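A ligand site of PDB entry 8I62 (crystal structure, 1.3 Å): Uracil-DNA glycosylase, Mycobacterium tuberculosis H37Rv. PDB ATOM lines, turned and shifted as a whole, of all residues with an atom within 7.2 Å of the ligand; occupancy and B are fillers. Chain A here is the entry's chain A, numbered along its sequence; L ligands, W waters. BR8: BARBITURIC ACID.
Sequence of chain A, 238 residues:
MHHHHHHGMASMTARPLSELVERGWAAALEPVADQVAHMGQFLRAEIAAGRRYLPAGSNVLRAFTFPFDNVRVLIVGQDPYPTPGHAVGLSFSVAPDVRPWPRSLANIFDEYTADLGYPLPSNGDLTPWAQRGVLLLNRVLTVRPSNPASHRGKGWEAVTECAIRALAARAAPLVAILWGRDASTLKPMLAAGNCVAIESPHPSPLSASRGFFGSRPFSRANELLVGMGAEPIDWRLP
Residues that only touch the ligand: Gly 77 (3.6 Å), Pro 80 (3.8 Å), Tyr 81 (3.2 Å) and Ser 91 (3.4 Å).
Hydrophobic or aromatic side chains within 4 Å of the ligand: Tyr 81, Phe 92 and His 202.
Within 4 Å of the ligand: Gly 77, Gln 78, Asp 79, Pro 80, Tyr 81, Ser 91, Phe 92, Asn 138 and His 202.
The nearest printed residue that does not touch the ligand is Pro 82 (4.1 Å).
The backbone NH (N) of Gln 78 lies within hydrogen-bond range of the side-chain amide oxygen (OD1) of Asn 138 (3.4 Å).
The side-chain carboxylate of Asp 79 sits close to the side-chain amide oxygen of Gln 78.
O of Gln 78 sits at hydrogen-bond distance from N of Arg 139, 3.3 Å away.
N of Ser 204 lies within hydrogen-bond range of ND1 of His 202 (2.9 Å).
The backbone carbonyl oxygen (O) of Phe 92 lies within hydrogen-bond range of the side-chain hydroxyl (OH) of Tyr 81 (2.7 Å).
OG of Ser 91 sits at hydrogen-bond distance from O of Leu 137, 3.1 Å away.
O of Leu 137 lies within hydrogen-bond range of N of Gly 77, at 3.0 Å.
O of Gly 77 is in hydrogen-bond range of N of Arg 139, 2.9 Å away.
Water W1 bridges an oxygen (O4) of the ligand (2.7 Å) and the backbone NH of Tyr 81 (3.0 Å).
Water W2 bridges N1 of the ligand (2.9 Å) and NE2 of His 202 (3.3 Å).
The backbone NH of Gln 78 sits at hydrogen-bond distance from an oxygen (O2) of the ligand (2.7 Å).
A ring nitrogen (NE2) of His 202 lies within hydrogen-bond range of an oxygen (O2) of the ligand, 2.8 Å away.
The backbone NH (N) of Phe 92 sits at hydrogen-bond distance from an oxygen (O4) of the ligand.
The side-chain amide oxygen (OD1) of Asn 138 sits at hydrogen-bond distance from a nitrogen (N3) of the ligand, at 2.9 Å.
N3 of the ligand sits at hydrogen-bond distance from O of Asp 79.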
ATOM      1  N   VAL A  76      -7.819   6.053 -15.206  1.00  0.00           N
ATOM      2  CA  VAL A  76      -7.565   5.659 -13.826  1.00  0.00           C
ATOM      3  C   VAL A  76      -7.392   4.154 -13.757  1.00  0.00           C
ATOM      4  O   VAL A  76      -8.332   3.397 -14.167  1.00  0.00           O
ATOM      5  CB  VAL A  76      -8.634   6.148 -12.867  1.00  0.00           C
ATOM      6  CG1 VAL A  76      -8.193   5.877 -11.438  1.00  0.00           C
ATOM      7  CG2 VAL A  76      -8.981   7.595 -13.065  1.00  0.00           C
ATOM      8  N   GLY A  77      -6.256   3.709 -13.257  1.00  0.00           N
ATOM      9  CA  GLY A  77      -6.049   2.323 -12.889  1.00  0.00           C
ATOM     10  C   GLY A  77      -6.051   2.103 -11.383  1.00  0.00           C
ATOM     11  O   GLY A  77      -6.653   2.911 -10.627  1.00  0.00           O
ATOM     12  N   GLN A  78      -5.474   0.990 -10.984  1.00  0.00           N
ATOM     13  CA  GLN A  78      -5.542   0.486  -9.607  1.00  0.00           C
ATOM     14  C   GLN A  78      -4.416   1.046  -8.728  1.00  0.00           C
ATOM     15  O   GLN A  78      -4.658   1.756  -7.744  1.00  0.00           O
ATOM     16  CB  GLN A  78      -5.516  -1.052  -9.618  1.00  0.00           C
ATOM     17  CG  GLN A  78      -5.476  -1.651  -8.225  1.00  0.00           C
ATOM     18  CD  GLN A  78      -5.422  -3.144  -8.224  1.00  0.00           C
ATOM     19  OE1 GLN A  78      -4.317  -3.734  -8.100  1.00  0.00           O
ATOM     20  NE2 GLN A  78      -6.567  -3.741  -8.365  1.00  0.00           N
ATOM     21  N   ASP A  79      -3.186   0.735  -9.118  1.00  0.00           N
ATOM     22  CA  ASP A  79      -1.982   1.051  -8.317  1.00  0.00           C
ATOM     23  C   ASP A  79      -0.787   0.812  -9.229  1.00  0.00           C
ATOM     24  O   ASP A  79      -0.947   0.266 -10.331  1.00  0.00           O
ATOM     25  CB  ASP A  79      -1.925   0.280  -7.007  1.00  0.00           C
ATOM     26  CG  ASP A  79      -1.672  -1.212  -7.071  1.00  0.00           C
ATOM     27  OD1 ASP A  79      -2.070  -1.816  -8.063  1.00  0.00           O
ATOM     28  OD2 ASP A  79      -1.113  -1.732  -6.080  1.00  0.00           O
ATOM     29  N   PRO A  80       0.421   1.254  -8.852  1.00  0.00           N
ATOM     30  CA  PRO A  80       1.521   1.191  -9.797  1.00  0.00           C
ATOM     31  C   PRO A  80       2.046  -0.215 -10.099  1.00  0.00           C
ATOM     32  O   PRO A  80       1.781  -1.164  -9.341  1.00  0.00           O
ATOM     33  CB  PRO A  80       2.650   1.991  -9.079  1.00  0.00           C
ATOM     34  CG  PRO A  80       1.883   2.937  -8.150  1.00  0.00           C
ATOM     35  CD  PRO A  80       0.706   2.074  -7.669  1.00  0.00           C
ATOM     36  N   TYR A  81       2.813  -0.304 -11.172  1.00  0.00           N
ATOM     37  CA  TYR A  81       3.423  -1.581 -11.521  1.00  0.00           C
ATOM     38  C   TYR A  81       4.179  -2.117 -10.347  1.00  0.00           C
ATOM     39  O   TYR A  81       4.954  -1.423  -9.690  1.00  0.00           O
ATOM     40  CB  TYR A  81       4.373  -1.482 -12.684  1.00  0.00           C
ATOM     41  CG  TYR A  81       3.744  -1.271 -14.015  1.00  0.00           C
ATOM     42  CD1 TYR A  81       2.942  -2.253 -14.594  1.00  0.00           C
ATOM     43  CD2 TYR A  81       3.941  -0.121 -14.743  1.00  0.00           C
ATOM     44  CE1 TYR A  81       2.324  -2.075 -15.824  1.00  0.00           C
ATOM     45  CE2 TYR A  81       3.401   0.055 -15.999  1.00  0.00           C
ATOM     46  CZ  TYR A  81       2.554  -0.911 -16.545  1.00  0.00           C
ATOM     47  OH  TYR A  81       1.963  -0.797 -17.756  1.00  0.00           O
ATOM     48  N   PRO A  82       4.092  -3.455 -10.046  1.00  0.00           N
ATOM     49  CA  PRO A  82       4.763  -4.026  -8.879  1.00  0.00           C
ATOM     50  C   PRO A  82       6.223  -4.417  -9.104  1.00  0.00           C
ATOM     51  O   PRO A  82       6.878  -4.759  -8.134  1.00  0.00           O
ATOM     52  CB  PRO A  82       3.905  -5.292  -8.609  1.00  0.00           C
ATOM     53  CG  PRO A  82       3.411  -5.710  -9.975  1.00  0.00           C
ATOM     54  CD  PRO A  82       3.104  -4.395 -10.646  1.00  0.00           C
ATOM     55  N   THR A  83       6.681  -4.438 -10.351  1.00  0.00           N
ATOM     56  CA  THR A  83       8.073  -4.882 -10.645  1.00  0.00           C
ATOM     57  C   THR A  83       9.008  -3.696 -10.612  1.00  0.00           C
ATOM     58  O   THR A  83       8.792  -2.714 -11.306  1.00  0.00           O
ATOM     59  CB  THR A  83       8.171  -5.535 -12.032  1.00  0.00           C
ATOM     60  OG1 THR A  83       7.106  -6.477 -12.139  1.00  0.00           O
ATOM     61  CG2 THR A  83       9.502  -6.225 -12.209  1.00  0.00           C
ATOM     62  N   ALA A  87       7.269   1.115 -12.800  1.00  0.00           N
ATOM     63  CA  ALA A  87       6.445   2.281 -12.479  1.00  0.00           C
ATOM     64  C   ALA A  87       7.240   3.586 -12.569  1.00  0.00           C
ATOM     65  O   ALA A  87       8.345   3.663 -11.998  1.00  0.00           O
ATOM     66  CB  ALA A  87       5.803   2.135 -11.136  1.00  0.00           C
ATOM     67  N   VAL A  88       6.600   4.597 -13.148  1.00  0.00           N
ATOM     68  CA  VAL A  88       7.231   5.929 -13.286  1.00  0.00           C
ATOM     69  C   VAL A  88       6.329   7.062 -12.810  1.00  0.00           C
ATOM     70  O   VAL A  88       6.681   8.220 -13.031  1.00  0.00           O
ATOM     71  CB  VAL A  88       7.684   6.185 -14.733  1.00  0.00           C
ATOM     72  CG1 VAL A  88       8.688   5.139 -15.197  1.00  0.00           C
ATOM     73  CG2 VAL A  88       6.494   6.266 -15.689  1.00  0.00           C
ATOM     74  N   GLY A  89       5.221   6.737 -12.128  1.00  0.00           N
ATOM     75  CA  GLY A  89       4.342   7.775 -11.589  1.00  0.00           C
ATOM     76  C   GLY A  89       3.262   8.259 -12.521  1.00  0.00           C
ATOM     77  O   GLY A  89       2.497   9.169 -12.185  1.00  0.00           O
ATOM     78  N   LEU A  90       3.227   7.725 -13.727  1.00  0.00           N
ATOM     79  CA  LEU A  90       2.145   7.934 -14.708  1.00  0.00           C
ATOM     80  C   LEU A  90       1.530   6.564 -14.936  1.00  0.00           C
ATOM     81  O   LEU A  90       2.256   5.637 -15.301  1.00  0.00           O
ATOM     82  CB  LEU A  90       2.666   8.487 -16.019  1.00  0.00           C
ATOM     83  CG  LEU A  90       3.283   9.851 -15.919  1.00  0.00           C
ATOM     84  CD1 LEU A  90       3.939  10.244 -17.211  1.00  0.00           C
ATOM     85  CD2 LEU A  90       2.306  10.943 -15.428  1.00  0.00           C
ATOM     86  N   SER A  91       0.241   6.408 -14.714  1.00  0.00           N
ATOM     87  CA  SER A  91      -0.362   5.064 -14.766  1.00  0.00           C
ATOM     88  C   SER A  91      -0.074   4.415 -16.113  1.00  0.00           C
ATOM     89  O   SER A  91      -0.160   5.049 -17.182  1.00  0.00           O
ATOM     90  CB  SER A  91      -1.787   5.086 -14.430  1.00  0.00           C
ATOM     91  OG  SER A  91      -2.546   5.832 -15.353  1.00  0.00           O
ATOM     92  N   PHE A  92       0.320   3.154 -16.008  1.00  0.00           N
ATOM     93  CA  PHE A  92       0.589   2.231 -17.122  1.00  0.00           C
ATOM     94  C   PHE A  92       1.826   2.524 -17.933  1.00  0.00           C
ATOM     95  O   PHE A  92       2.263   1.690 -18.714  1.00  0.00           O
ATOM     96  CB  PHE A  92      -0.642   2.038 -18.023  1.00  0.00           C
ATOM     97  CG  PHE A  92      -1.824   1.538 -17.256  1.00  0.00           C
ATOM     98  CD1 PHE A  92      -1.917   0.212 -16.898  1.00  0.00           C
ATOM     99  CD2 PHE A  92      -2.812   2.415 -16.832  1.00  0.00           C
ATOM    100  CE1 PHE A  92      -3.008  -0.265 -16.180  1.00  0.00           C
ATOM    101  CE2 PHE A  92      -3.868   1.944 -16.077  1.00  0.00           C
ATOM    102  CZ  PHE A  92      -3.992   0.602 -15.784  1.00  0.00           C
ATOM    103  N   SER A  93       2.434   3.703 -17.773  1.00  0.00           N
ATOM    104  CA  SER A  93       3.593   4.094 -18.585  1.00  0.00           C
ATOM    105  C   SER A  93       4.869   3.379 -18.124  1.00  0.00           C
ATOM    106  O   SER A  93       5.008   3.101 -16.916  1.00  0.00           O
ATOM    107  CB  SER A  93       3.773   5.612 -18.510  1.00  0.00           C
ATOM    108  OG  SER A  93       4.604   6.095 -19.520  1.00  0.00           O
ATOM    109  N   PRO A 102       5.282  -4.450 -19.822  1.00  0.00           N
ATOM    110  CA  PRO A 102       4.384  -5.160 -18.909  1.00  0.00           C
ATOM    111  C   PRO A 102       3.167  -5.706 -19.657  1.00  0.00           C
ATOM    112  O   PRO A 102       2.671  -5.116 -20.650  1.00  0.00           O
ATOM    113  CB  PRO A 102       3.999  -4.084 -17.885  1.00  0.00           C
ATOM    114  CG  PRO A 102       5.101  -3.118 -17.963  1.00  0.00           C
ATOM    115  CD  PRO A 102       5.568  -3.083 -19.397  1.00  0.00           C
ATOM    116  N   SER A 104      -0.017  -5.815 -18.899  1.00  0.00           N
ATOM    117  CA  SER A 104      -1.178  -4.885 -18.936  1.00  0.00           C
ATOM    118  C   SER A 104      -1.003  -3.879 -20.075  1.00  0.00           C
ATOM    119  O   SER A 104      -1.978  -3.542 -20.770  1.00  0.00           O
ATOM    120  CB  SER A 104      -1.398  -4.157 -17.627  1.00  0.00           C
ATOM    121  OG  SER A 104      -1.990  -5.000 -16.678  1.00  0.00           O
ATOM    122  N   LEU A 136      -2.896  10.538 -16.217  1.00  0.00           N
ATOM    123  CA  LEU A 136      -2.604   9.096 -16.084  1.00  0.00           C
ATOM    124  C   LEU A 136      -2.510   8.774 -14.592  1.00  0.00           C
ATOM    125  O   LEU A 136      -1.427   8.715 -13.986  1.00  0.00           O
ATOM    126  CB  LEU A 136      -1.309   8.799 -16.849  1.00  0.00           C
ATOM    127  CG  LEU A 136      -1.365   9.083 -18.332  1.00  0.00           C
ATOM    128  CD1 LEU A 136      -0.038   8.838 -18.992  1.00  0.00           C
ATOM    129  CD2 LEU A 136      -2.412   8.234 -18.988  1.00  0.00           C
ATOM    130  N   LEU A 137      -3.670   8.520 -14.007  1.00  0.00           N
ATOM    131  CA  LEU A 137      -3.831   8.372 -12.558  1.00  0.00           C
ATOM    132  C   LEU A 137      -3.994   6.901 -12.174  1.00  0.00           C
ATOM    133  O   LEU A 137      -4.495   6.082 -12.981  1.00  0.00           O
ATOM    134  CB  LEU A 137      -5.061   9.151 -12.129  1.00  0.00           C
ATOM    135  CG  LEU A 137      -5.197   9.427 -10.645  1.00  0.00           C
ATOM    136  CD1 LEU A 137      -4.036  10.260 -10.127  1.00  0.00           C
ATOM    137  CD2 LEU A 137      -6.529  10.100 -10.375  1.00  0.00           C
ATOM    138  N   ASN A 138      -3.581   6.550 -10.983  1.00  0.00           N
ATOM    139  CA  ASN A 138      -3.954   5.326 -10.292  1.00  0.00           C
ATOM    140  C   ASN A 138      -4.778   5.682  -9.071  1.00  0.00           C
ATOM    141  O   ASN A 138      -4.535   6.741  -8.447  1.00  0.00           O
ATOM    142  CB  ASN A 138      -2.750   4.455  -9.938  1.00  0.00           C
ATOM    143  CG  ASN A 138      -2.165   3.712 -11.117  1.00  0.00           C
ATOM    144  OD1 ASN A 138      -2.957   3.080 -11.869  1.00  0.00           O
ATOM    145  ND2 ASN A 138      -0.855   3.727 -11.309  1.00  0.00           N
ATOM    146  N   ARG A 139      -5.683   4.807  -8.660  1.00  0.00           N
ATOM    147  CA  ARG A 139      -6.500   5.090  -7.457  1.00  0.00           C
ATOM    148  C   ARG A 139      -5.596   5.201  -6.242  1.00  0.00           C
ATOM    149  O   ARG A 139      -5.888   5.994  -5.320  1.00  0.00           O
ATOM    150  CB  ARG A 139      -7.557   3.994  -7.321  1.00  0.00           C
ATOM    151  CG  ARG A 139      -8.610   4.256  -6.279  1.00  0.00           C
ATOM    152  CD  ARG A 139      -9.589   5.365  -6.710  1.00  0.00           C
ATOM    153  NE  ARG A 139     -10.734   5.406  -5.843  1.00  0.00           N
ATOM    154  CZ  ARG A 139     -10.851   6.183  -4.774  1.00  0.00           C
ATOM    155  NH1 ARG A 139      -9.946   7.122  -4.509  1.00  0.00           N
ATOM    156  NH2 ARG A 139     -11.890   6.023  -3.986  1.00  0.00           N
ATOM    157  N   VAL A 140      -4.555   4.375  -6.185  1.00  0.00           N
ATOM    158  CA  VAL A 140      -3.556   4.311  -5.107  1.00  0.00           C
ATOM    159  C   VAL A 140      -2.219   4.544  -5.799  1.00  0.00           C
ATOM    160  O   VAL A 140      -1.948   4.025  -6.863  1.00  0.00           O
ATOM    161  CB  VAL A 140      -3.659   2.949  -4.401  1.00  0.00           C
ATOM    162  CG1 VAL A 140      -2.458   2.675  -3.498  1.00  0.00           C
ATOM    163  CG2 VAL A 140      -4.974   2.904  -3.612  1.00  0.00           C
ATOM    164  N   PRO A 148       0.982  -6.473  -5.777  1.00  0.00           N
ATOM    165  CA  PRO A 148      -0.119  -5.609  -6.206  1.00  0.00           C
ATOM    166  C   PRO A 148      -1.128  -5.399  -5.082  1.00  0.00           C
ATOM    167  O   PRO A 148      -1.470  -6.326  -4.348  1.00  0.00           O
ATOM    168  CB  PRO A 148      -0.750  -6.331  -7.389  1.00  0.00           C
ATOM    169  CG  PRO A 148       0.322  -7.223  -7.895  1.00  0.00           C
ATOM    170  CD  PRO A 148       1.191  -7.605  -6.718  1.00  0.00           C
ATOM    171  N   TRP A 179     -10.630   1.931 -15.284  1.00  0.00           N
ATOM    172  CA  TRP A 179     -10.211   0.538 -15.541  1.00  0.00           C
ATOM    173  C   TRP A 179     -10.136  -0.237 -14.245  1.00  0.00           C
ATOM    174  O   TRP A 179      -9.205  -0.021 -13.438  1.00  0.00           O
ATOM    175  CB  TRP A 179      -8.902   0.506 -16.305  1.00  0.00           C
ATOM    176  CG  TRP A 179      -9.001   0.894 -17.751  1.00  0.00           C
ATOM    177  CD1 TRP A 179     -10.117   0.831 -18.543  1.00  0.00           C
ATOM    178  CD2 TRP A 179      -7.938   1.331 -18.582  1.00  0.00           C
ATOM    179  NE1 TRP A 179      -9.804   1.258 -19.810  1.00  0.00           N
ATOM    180  CE2 TRP A 179      -8.488   1.588 -19.864  1.00  0.00           C
ATOM    181  CE3 TRP A 179      -6.586   1.573 -18.389  1.00  0.00           C
ATOM    182  CZ2 TRP A 179      -7.717   2.053 -20.937  1.00  0.00           C
ATOM    183  CZ3 TRP A 179      -5.828   2.012 -19.426  1.00  0.00           C
ATOM    184  CH2 TRP A 179      -6.376   2.283 -20.673  1.00  0.00           C
ATOM    185  N   HIS A 202     -10.334  -4.154 -16.021  1.00  0.00           N
ATOM    186  CA  HIS A 202      -8.934  -3.706 -16.128  1.00  0.00           C
ATOM    187  C   HIS A 202      -8.169  -4.499 -17.193  1.00  0.00           C
ATOM    188  O   HIS A 202      -8.455  -5.680 -17.415  1.00  0.00           O
ATOM    189  CB  HIS A 202      -8.352  -3.877 -14.716  1.00  0.00           C
ATOM    190  CG  HIS A 202      -6.986  -3.334 -14.467  1.00  0.00           C
ATOM    191  ND1 HIS A 202      -5.877  -4.003 -14.934  1.00  0.00           N
ATOM    192  CD2 HIS A 202      -6.610  -2.247 -13.735  1.00  0.00           C
ATOM    193  CE1 HIS A 202      -4.823  -3.315 -14.482  1.00  0.00           C
ATOM    194  NE2 HIS A 202      -5.245  -2.240 -13.735  1.00  0.00           N
ATOM    195  N   PRO A 203      -7.146  -3.892 -17.821  1.00  0.00           N
ATOM    196  CA  PRO A 203      -6.359  -4.587 -18.848  1.00  0.00           C
ATOM    197  C   PRO A 203      -5.389  -5.654 -18.370  1.00  0.00           C
ATOM    198  O   PRO A 203      -4.782  -6.323 -19.190  1.00  0.00           O
ATOM    199  CB  PRO A 203      -5.614  -3.450 -19.553  1.00  0.00           C
ATOM    200  CG  PRO A 203      -5.517  -2.358 -18.488  1.00  0.00           C
ATOM    201  CD  PRO A 203      -6.833  -2.473 -17.766  1.00  0.00           C
ATOM    202  N   SER A 204      -5.259  -5.820 -17.047  1.00  0.00           N
ATOM    203  CA  SER A 204      -4.497  -6.957 -16.507  1.00  0.00           C
ATOM    204  C   SER A 204      -4.907  -8.242 -17.223  1.00  0.00           C
ATOM    205  O   SER A 204      -6.131  -8.481 -17.363  1.00  0.00           O
ATOM    206  CB  SER A 204      -4.769  -7.116 -15.026  1.00  0.00           C
ATOM    207  OG  SER A 204      -4.234  -8.352 -14.579  1.00  0.00           O
HETATM  208  N1  BR8 L   1      -1.731  -1.539 -12.913  1.00  0.00           N
HETATM  209  C2  BR8 L   1      -2.471  -0.385 -12.816  1.00  0.00           C
HETATM  210  O2  BR8 L   1      -3.648  -0.370 -12.487  1.00  0.00           O
HETATM  211  N3  BR8 L   1      -1.778   0.760 -13.056  1.00  0.00           N
HETATM  212  C4  BR8 L   1      -0.440   0.836 -13.343  1.00  0.00           C
HETATM  213  O4  BR8 L   1       0.125   1.938 -13.436  1.00  0.00           O
HETATM  214  C5  BR8 L   1       0.302  -0.395 -13.479  1.00  0.00           C
HETATM  215  C6  BR8 L   1      -0.393  -1.631 -13.100  1.00  0.00           C
HETATM  216  O8  BR8 L   1       0.218  -2.713 -12.942  1.00  0.00           O
HETATM  217  O   HOH W   1       2.729   2.270 -12.711  1.00  0.00           O
HETATM  218  O   HOH W   2      -3.038  -3.881 -11.876  1.00  0.00           O
HETATM  219  O   HOH W   3      -0.439  -4.546 -10.973  1.00  0.00           O
